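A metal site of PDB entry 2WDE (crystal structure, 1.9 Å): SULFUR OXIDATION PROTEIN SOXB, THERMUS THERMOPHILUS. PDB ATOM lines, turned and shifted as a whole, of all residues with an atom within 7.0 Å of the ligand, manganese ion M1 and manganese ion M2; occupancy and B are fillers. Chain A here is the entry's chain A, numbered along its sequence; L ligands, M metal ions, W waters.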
ATOM      1  N   SER A  35      -6.898 -15.784  13.400  1.00  0.00           N
ATOM      2  CA  SER A  35      -6.672 -17.219  13.257  1.00  0.00           C
ATOM      3  C   SER A  35      -5.367 -17.439  12.549  1.00  0.00           C
ATOM      4  O   SER A  35      -4.837 -16.525  11.913  1.00  0.00           O
ATOM      5  CB  SER A  35      -7.808 -17.841  12.429  1.00  0.00           C
ATOM      6  OG  SER A  35      -7.714 -19.257  12.406  1.00  0.00           O
ATOM      7  N   ASP A  36      -4.839 -18.652  12.677  1.00  0.00           N
ATOM      8  CA  ASP A  36      -3.625 -19.035  11.971  1.00  0.00           C
ATOM      9  C   ASP A  36      -2.412 -18.113  12.199  1.00  0.00           C
ATOM     10  O   ASP A  36      -1.653 -17.787  11.269  1.00  0.00           O
ATOM     11  CB  ASP A  36      -3.925 -19.218  10.482  1.00  0.00           C
ATOM     12  CG  ASP A  36      -4.909 -20.370  10.224  1.00  0.00           C
ATOM     13  OD1 ASP A  36      -4.473 -21.528  10.026  1.00  0.00           O
ATOM     14  OD2 ASP A  36      -6.138 -20.120  10.237  1.00  0.00           O
ATOM     15  N   LEU A  37      -2.215 -17.724  13.447  1.00  0.00           N
ATOM     16  CA  LEU A  37      -1.089 -16.884  13.811  1.00  0.00           C
ATOM     17  C   LEU A  37       0.216 -17.636  13.543  1.00  0.00           C
ATOM     18  O   LEU A  37       1.221 -17.047  13.168  1.00  0.00           O
ATOM     19  CB  LEU A  37      -1.164 -16.482  15.292  1.00  0.00           C
ATOM     20  CG  LEU A  37      -0.024 -15.645  15.866  1.00  0.00           C
ATOM     21  CD1 LEU A  37       0.144 -14.312  15.176  1.00  0.00           C
ATOM     22  CD2 LEU A  37      -0.243 -15.438  17.363  1.00  0.00           C
ATOM     23  N   HIS A  38       0.185 -18.958  13.698  1.00  0.00           N
ATOM     24  CA  HIS A  38       1.376 -19.786  13.486  1.00  0.00           C
ATOM     25  C   HIS A  38       2.604 -19.254  14.234  1.00  0.00           C
ATOM     26  O   HIS A  38       3.686 -19.084  13.666  1.00  0.00           O
ATOM     27  CB  HIS A  38       1.644 -19.978  11.981  1.00  0.00           C
ATOM     28  CG  HIS A  38       0.723 -20.966  11.341  1.00  0.00           C
ATOM     29  ND1 HIS A  38       0.951 -22.325  11.372  1.00  0.00           N
ATOM     30  CD2 HIS A  38      -0.419 -20.803  10.640  1.00  0.00           C
ATOM     31  CE1 HIS A  38      -0.011 -22.956  10.732  1.00  0.00           C
ATOM     32  NE2 HIS A  38      -0.860 -22.057  10.270  1.00  0.00           N
ATOM     33  N   GLY A 130      -8.872 -18.810  16.059  1.00  0.00           N
ATOM     34  CA  GLY A 130      -9.212 -19.875  15.135  1.00  0.00           C
ATOM     35  C   GLY A 130      -8.276 -21.067  15.054  1.00  0.00           C
ATOM     36  O   GLY A 130      -8.550 -22.003  14.309  1.00  0.00           O
ATOM     37  N   GLY A 131      -7.179 -21.071  15.803  1.00  0.00           N
ATOM     38  CA  GLY A 131      -6.270 -22.217  15.783  1.00  0.00           C
ATOM     39  C   GLY A 131      -5.064 -22.053  14.865  1.00  0.00           C
ATOM     40  O   GLY A 131      -4.916 -21.021  14.199  1.00  0.00           O
ATOM     41  N   ASP A 132      -4.193 -23.067  14.851  1.00  0.00           N
ATOM     42  CA  ASP A 132      -2.922 -22.989  14.122  1.00  0.00           C
ATOM     43  C   ASP A 132      -2.192 -21.814  14.733  1.00  0.00           C
ATOM     44  O   ASP A 132      -1.630 -20.962  14.052  1.00  0.00           O
ATOM     45  CB  ASP A 132      -3.115 -22.797  12.620  1.00  0.00           C
ATOM     46  CG  ASP A 132      -3.261 -24.112  11.894  1.00  0.00           C
ATOM     47  OD1 ASP A 132      -3.312 -25.149  12.606  1.00  0.00           O
ATOM     48  OD2 ASP A 132      -3.390 -24.119  10.658  1.00  0.00           O
ATOM     49  N   THR A 133      -2.232 -21.795  16.058  1.00  0.00           N
ATOM     50  CA  THR A 133      -1.636 -20.727  16.840  1.00  0.00           C
ATOM     51  C   THR A 133      -0.302 -21.067  17.511  1.00  0.00           C
ATOM     52  O   THR A 133       0.613 -20.244  17.521  1.00  0.00           O
ATOM     53  CB  THR A 133      -2.631 -20.310  17.959  1.00  0.00           C
ATOM     54  OG1 THR A 133      -3.920 -20.069  17.389  1.00  0.00           O
ATOM     55  CG2 THR A 133      -2.135 -19.059  18.684  1.00  0.00           C
ATOM     56  N   ASN A 136       4.926 -23.579  14.651  1.00  0.00           N
ATOM     57  CA  ASN A 136       5.592 -23.016  13.471  1.00  0.00           C
ATOM     58  C   ASN A 136       6.276 -21.656  13.565  1.00  0.00           C
ATOM     59  O   ASN A 136       6.082 -20.799  12.699  1.00  0.00           O
ATOM     60  CB  ASN A 136       4.636 -23.084  12.285  1.00  0.00           C
ATOM     61  CG  ASN A 136       3.785 -24.347  12.309  1.00  0.00           C
ATOM     62  OD1 ASN A 136       2.575 -24.274  12.503  1.00  0.00           O
ATOM     63  ND2 ASN A 136       4.426 -25.503  12.152  1.00  0.00           N
ATOM     64  N   SER A 162      -8.467 -25.922  17.115  1.00  0.00           N
ATOM     65  CA  SER A 162      -7.123 -26.405  16.780  1.00  0.00           C
ATOM     66  C   SER A 162      -6.938 -27.105  15.452  1.00  0.00           C
ATOM     67  O   SER A 162      -7.891 -27.558  14.789  1.00  0.00           O
ATOM     68  CB  SER A 162      -6.701 -27.399  17.871  1.00  0.00           C
ATOM     69  OG  SER A 162      -7.403 -28.632  17.695  1.00  0.00           O
ATOM     70  N   HIS A 163      -5.663 -27.265  15.107  1.00  0.00           N
ATOM     71  CA  HIS A 163      -5.221 -28.038  13.961  1.00  0.00           C
ATOM     72  C   HIS A 163      -3.763 -28.405  14.180  1.00  0.00           C
ATOM     73  O   HIS A 163      -3.466 -29.473  14.744  1.00  0.00           O
ATOM     74  CB  HIS A 163      -5.415 -27.320  12.622  1.00  0.00           C
ATOM     75  CG  HIS A 163      -4.726 -28.007  11.480  1.00  0.00           C
ATOM     76  ND1 HIS A 163      -4.520 -27.417  10.252  1.00  0.00           N
ATOM     77  CD2 HIS A 163      -4.177 -29.244  11.387  1.00  0.00           C
ATOM     78  CE1 HIS A 163      -3.859 -28.242   9.468  1.00  0.00           C
ATOM     79  NE2 HIS A 163      -3.663 -29.371  10.123  1.00  0.00           N
ATOM     80  N   TRP A 164      -2.854 -27.508  13.802  1.00  0.00           N
ATOM     81  CA  TRP A 164      -1.410 -27.755  13.936  1.00  0.00           C
ATOM     82  C   TRP A 164      -0.933 -27.904  15.383  1.00  0.00           C
ATOM     83  O   TRP A 164       0.172 -28.400  15.641  1.00  0.00           O
ATOM     84  CB  TRP A 164      -0.603 -26.676  13.193  1.00  0.00           C
ATOM     85  CG  TRP A 164      -0.428 -26.956  11.705  1.00  0.00           C
ATOM     86  CD1 TRP A 164      -1.306 -26.652  10.697  1.00  0.00           C
ATOM     87  CD2 TRP A 164       0.685 -27.597  11.084  1.00  0.00           C
ATOM     88  NE1 TRP A 164      -0.779 -27.038   9.480  1.00  0.00           N
ATOM     89  CE2 TRP A 164       0.430 -27.633   9.698  1.00  0.00           C
ATOM     90  CE3 TRP A 164       1.889 -28.141  11.564  1.00  0.00           C
ATOM     91  CZ2 TRP A 164       1.305 -28.245   8.784  1.00  0.00           C
ATOM     92  CZ3 TRP A 164       2.773 -28.724  10.649  1.00  0.00           C
ATOM     93  CH2 TRP A 164       2.469 -28.754   9.278  1.00  0.00           C
ATOM     94  N   TYR A 219      -9.829 -28.967  12.854  1.00  0.00           N
ATOM     95  CA  TYR A 219      -9.558 -29.517  11.521  1.00  0.00           C
ATOM     96  C   TYR A 219      -9.854 -31.024  11.511  1.00  0.00           C
ATOM     97  O   TYR A 219      -9.321 -31.768  12.333  1.00  0.00           O
ATOM     98  CB  TYR A 219      -8.097 -29.251  11.133  1.00  0.00           C
ATOM     99  CG  TYR A 219      -7.748 -29.588   9.710  1.00  0.00           C
ATOM    100  CD1 TYR A 219      -8.465 -29.044   8.649  1.00  0.00           C
ATOM    101  CD2 TYR A 219      -6.679 -30.419   9.408  1.00  0.00           C
ATOM    102  CE1 TYR A 219      -8.159 -29.359   7.332  1.00  0.00           C
ATOM    103  CE2 TYR A 219      -6.350 -30.717   8.107  1.00  0.00           C
ATOM    104  CZ  TYR A 219      -7.082 -30.194   7.082  1.00  0.00           C
ATOM    105  OH  TYR A 219      -6.739 -30.499   5.787  1.00  0.00           O
ATOM    106  N   HIS A 226      -0.656 -35.344   9.286  1.00  0.00           N
ATOM    107  CA  HIS A 226       0.516 -35.297  10.155  1.00  0.00           C
ATOM    108  C   HIS A 226       0.818 -36.686  10.701  1.00  0.00           C
ATOM    109  O   HIS A 226      -0.032 -37.562  10.606  1.00  0.00           O
ATOM    110  CB  HIS A 226       0.234 -34.348  11.320  1.00  0.00           C
ATOM    111  CG  HIS A 226      -0.375 -33.058  10.885  1.00  0.00           C
ATOM    112  ND1 HIS A 226       0.374 -32.021  10.364  1.00  0.00           N
ATOM    113  CD2 HIS A 226      -1.668 -32.635  10.856  1.00  0.00           C
ATOM    114  CE1 HIS A 226      -0.430 -31.029  10.027  1.00  0.00           C
ATOM    115  NE2 HIS A 226      -1.674 -31.365  10.324  1.00  0.00           N
ATOM    116  N   HIS A 263     -12.118 -24.544  12.098  1.00  0.00           N
ATOM    117  CA  HIS A 263     -10.830 -24.790  11.467  1.00  0.00           C
ATOM    118  C   HIS A 263     -11.029 -25.907  10.463  1.00  0.00           C
ATOM    119  O   HIS A 263     -10.138 -26.726  10.239  1.00  0.00           O
ATOM    120  CB  HIS A 263      -9.707 -25.100  12.469  1.00  0.00           C
ATOM    121  CG  HIS A 263      -8.339 -24.816  11.944  1.00  0.00           C
ATOM    122  ND1 HIS A 263      -7.579 -23.740  12.359  1.00  0.00           N
ATOM    123  CD2 HIS A 263      -7.616 -25.417  10.958  1.00  0.00           C
ATOM    124  CE1 HIS A 263      -6.443 -23.718  11.693  1.00  0.00           C
ATOM    125  NE2 HIS A 263      -6.428 -24.733  10.850  1.00  0.00           N
ATOM    126  N   GLY A 285     -11.326 -20.405   9.815  1.00  0.00           N
ATOM    127  CA  GLY A 285      -9.876 -20.450   9.860  1.00  0.00           C
ATOM    128  C   GLY A 285      -9.367 -21.471   8.836  1.00  0.00           C
ATOM    129  O   GLY A 285     -10.110 -21.878   7.953  1.00  0.00           O
ATOM    130  N   HIS A 286      -8.103 -21.880   8.977  1.00  0.00           N
ATOM    131  CA  HIS A 286      -7.437 -22.897   8.146  1.00  0.00           C
ATOM    132  C   HIS A 286      -7.022 -22.512   6.738  1.00  0.00           C
ATOM    133  O   HIS A 286      -5.896 -22.813   6.321  1.00  0.00           O
ATOM    134  CB  HIS A 286      -8.217 -24.207   8.107  1.00  0.00           C
ATOM    135  CG  HIS A 286      -7.516 -25.293   7.346  1.00  0.00           C
ATOM    136  ND1 HIS A 286      -6.312 -25.850   7.768  1.00  0.00           N
ATOM    137  CD2 HIS A 286      -7.830 -25.930   6.198  1.00  0.00           C
ATOM    138  CE1 HIS A 286      -5.917 -26.747   6.889  1.00  0.00           C
ATOM    139  NE2 HIS A 286      -6.822 -26.828   5.929  1.00  0.00           N
ATOM    140  N   THR A 287      -7.929 -21.904   5.976  1.00  0.00           N
ATOM    141  CA  THR A 287      -7.592 -21.548   4.606  1.00  0.00           C
ATOM    142  C   THR A 287      -6.820 -20.233   4.467  1.00  0.00           C
ATOM    143  O   THR A 287      -6.411 -19.875   3.368  1.00  0.00           O
ATOM    144  CB  THR A 287      -8.806 -21.635   3.662  1.00  0.00           C
ATOM    145  OG1 THR A 287      -9.971 -21.156   4.335  1.00  0.00           O
ATOM    146  CG2 THR A 287      -9.033 -23.107   3.246  1.00  0.00           C
ATOM    147  N   HIS A 288      -6.601 -19.552   5.593  1.00  0.00           N
ATOM    148  CA  HIS A 288      -5.824 -18.302   5.601  1.00  0.00           C
ATOM    149  C   HIS A 288      -6.457 -17.224   4.701  1.00  0.00           C
ATOM    150  O   HIS A 288      -5.769 -16.402   4.108  1.00  0.00           O
ATOM    151  CB  HIS A 288      -4.358 -18.572   5.174  1.00  0.00           C
ATOM    152  CG  HIS A 288      -3.568 -19.382   6.159  1.00  0.00           C
ATOM    153  ND1 HIS A 288      -2.197 -19.272   6.284  1.00  0.00           N
ATOM    154  CD2 HIS A 288      -3.947 -20.322   7.063  1.00  0.00           C
ATOM    155  CE1 HIS A 288      -1.771 -20.118   7.204  1.00  0.00           C
ATOM    156  NE2 HIS A 288      -2.808 -20.758   7.701  1.00  0.00           N
ATOM    157  N   SER A 306      -7.857 -14.875   8.301  1.00  0.00           N
ATOM    158  CA  SER A 306      -6.573 -14.408   7.771  1.00  0.00           C
ATOM    159  C   SER A 306      -5.437 -15.237   8.357  1.00  0.00           C
ATOM    160  O   SER A 306      -5.604 -16.443   8.561  1.00  0.00           O
ATOM    161  CB  SER A 306      -6.363 -12.917   8.057  1.00  0.00           C
ATOM    162  OG  SER A 306      -5.262 -12.413   7.317  1.00  0.00           O
ATOM    163  N   ALA A 307      -4.295 -14.611   8.655  1.00  0.00           N
ATOM    164  CA  ALA A 307      -3.165 -15.383   9.145  1.00  0.00           C
ATOM    165  C   ALA A 307      -1.921 -14.590   9.538  1.00  0.00           C
ATOM    166  O   ALA A 307      -1.745 -13.437   9.145  1.00  0.00           O
ATOM    167  CB  ALA A 307      -2.782 -16.437   8.106  1.00  0.00           C
ATOM    168  N   ALA A 403       3.369 -27.623   0.292  1.00  0.00           N
ATOM    169  CA  ALA A 403       2.580 -26.434   0.013  1.00  0.00           C
ATOM    170  C   ALA A 403       1.724 -25.993   1.184  1.00  0.00           C
ATOM    171  O   ALA A 403       0.520 -25.765   1.040  1.00  0.00           O
ATOM    172  CB  ALA A 403       1.740 -26.643  -1.240  1.00  0.00           C
ATOM    173  N   VAL A 404       2.347 -25.871   2.356  1.00  0.00           N
ATOM    174  CA  VAL A 404       1.645 -25.357   3.533  1.00  0.00           C
ATOM    175  C   VAL A 404       1.296 -23.880   3.285  1.00  0.00           C
ATOM    176  O   VAL A 404       1.917 -23.222   2.448  1.00  0.00           O
ATOM    177  CB  VAL A 404       2.466 -25.553   4.837  1.00  0.00           C
ATOM    178  CG1 VAL A 404       2.699 -27.044   5.098  1.00  0.00           C
ATOM    179  CG2 VAL A 404       3.798 -24.783   4.781  1.00  0.00           C
ATOM    180  N   ARG A 405       0.286 -23.391   4.005  1.00  0.00           N
ATOM    181  CA  ARG A 405      -0.198 -22.015   3.911  1.00  0.00           C
ATOM    182  C   ARG A 405       0.541 -21.054   4.849  1.00  0.00           C
ATOM    183  O   ARG A 405       0.400 -19.846   4.739  1.00  0.00           O
ATOM    184  CB  ARG A 405      -1.683 -21.989   4.306  1.00  0.00           C
ATOM    185  CG  ARG A 405      -2.592 -22.684   3.312  1.00  0.00           C
ATOM    186  CD  ARG A 405      -4.064 -22.341   3.574  1.00  0.00           C
ATOM    187  NE  ARG A 405      -4.915 -22.999   2.589  1.00  0.00           N
ATOM    188  CZ  ARG A 405      -5.318 -24.264   2.670  1.00  0.00           C
ATOM    189  NH1 ARG A 405      -5.003 -24.994   3.733  1.00  0.00           N
ATOM    190  NH2 ARG A 405      -6.049 -24.804   1.719  1.00  0.00           N
ATOM    191  N   TRP A 406       1.252 -21.614   5.820  1.00  0.00           N
ATOM    192  CA  TRP A 406       2.001 -20.794   6.740  1.00  0.00           C
ATOM    193  C   TRP A 406       3.391 -20.435   6.198  1.00  0.00           C
ATOM    194  O   TRP A 406       3.932 -21.119   5.321  1.00  0.00           O
ATOM    195  CB  TRP A 406       2.106 -21.446   8.129  1.00  0.00           C
ATOM    196  CG  TRP A 406       2.481 -22.908   8.158  1.00  0.00           C
ATOM    197  CD1 TRP A 406       1.630 -23.970   8.146  1.00  0.00           C
ATOM    198  CD2 TRP A 406       3.784 -23.436   8.446  1.00  0.00           C
ATOM    199  NE1 TRP A 406       2.332 -25.139   8.321  1.00  0.00           N
ATOM    200  CE2 TRP A 406       3.656 -24.840   8.505  1.00  0.00           C
ATOM    201  CE3 TRP A 406       5.061 -22.870   8.546  1.00  0.00           C
ATOM    202  CZ2 TRP A 406       4.757 -25.681   8.707  1.00  0.00           C
ATOM    203  CZ3 TRP A 406       6.150 -23.710   8.760  1.00  0.00           C
ATOM    204  CH2 TRP A 406       5.991 -25.096   8.826  1.00  0.00           C
HETATM  205  S1  LIG L   1      -2.368 -25.000   7.137  1.00  0.00           S
HETATM  206  O1  LIG L   1      -3.009 -25.922   8.052  1.00  0.00           O
HETATM  207  O2  LIG L   1      -1.675 -23.905   7.817  1.00  0.00           O
HETATM  208  O3  LIG L   1      -3.272 -24.531   6.093  1.00  0.00           O
HETATM  209  S2  LIG L   1      -0.912 -26.057   6.191  1.00  0.00           S
HETATM  210 MN    MN M   1      -4.816 -25.360   9.472  1.00  0.00          MN
HETATM  211 MN    MN M   2      -2.767 -22.457   9.195  1.00  0.00          MN
HETATM  212  O   HOH W   1      -4.216 -23.444   8.302  1.00  0.00           O
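Manganese ion M1 is bound by a ring nitrogen (NE2) of His 263, a ring nitrogen (ND1) of His 163, the side-chain carboxylate (OD2) of Asp 132, a ring nitrogen (ND1) of His 286, water W1 and an oxygen (O1) of the ligand. Manganese ion M1 has six donor atoms within binding distance.
Val 404 touches the ligand. Trp 406 touches the ligand (CD1 to O2, 3.3 Å). The nearest printed residue that does not touch the ligand is Asp 36 (4.3 Å).
Four residues have an atom within 4 Å of manganese ion M2: Asp 36, His 38, Asp 132 and His 288. Along chain A the residues within 4 Å of manganese ion M2 span positions 36 to 288.
Water W1 lies within hydrogen-bond range of an oxygen (O3) of the ligand (2.6 Å) and the backbone carbonyl oxygen (O) of His 286 (2.7 Å).
Manganese ion M2 is bound by water W1 (2.0 Å), the side-chain carboxylate of Asp 36 (2.1 Å), a ring nitrogen (NE2) of His 38 (2.2 Å), a ring nitrogen (NE2) of His 288 (2.3 Å), an oxygen (O2) of the ligand (2.3 Å) and the side-chain carboxylate of Asp 132 (2.3 Å).
Merely in contact with manganese ion M1: Trp 164. Of the 25 residues printed, 6 come within 4 Å of manganese ion M1.
The side-chain carboxylate (OD2) of Asp 36 is in hydrogen-bond range of the side-chain hydroxyl (OG) of Ser 35, 2.8 Å away. The backbone carbonyl oxygen of Gly 131 is in hydrogen-bond range of the backbone NH of Asp 36, at 2.8 Å. A ring nitrogen (ND1) of His 38 is in hydrogen-bond range of the side-chain amide oxygen (OD1) of Asn 136 (2.8 Å). A ring nitrogen (NE2) of His 286 sits at hydrogen-bond distance from the guanidinium group (NH1) of Arg 405 (3.4 Å). The side-chain carboxylate (OD1) of Asp 132 lies within hydrogen-bond range of the backbone NH (N) of Trp 164 (2.7 Å). NE2 of His 226 lies within hydrogen-bond range of NE2 of His 163 (2.8 Å). N of His 286 sits at hydrogen-bond distance from OD2 of Asp 36, 2.9 Å away. The backbone carbonyl oxygen of Asp 132 is in hydrogen-bond range of the backbone NH of Leu 37 (3.3 Å).
O3 of the ligand is in salt-bridge range of NH1 of Arg 405 (3.0 Å). The indole nitrogen of Trp 164 lies close to a sulfur (S2) of the ligand (3.4 Å). The backbone NH of Arg 405 sits close to a sulfur (S2) of the ligand, at 3.6 Å.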
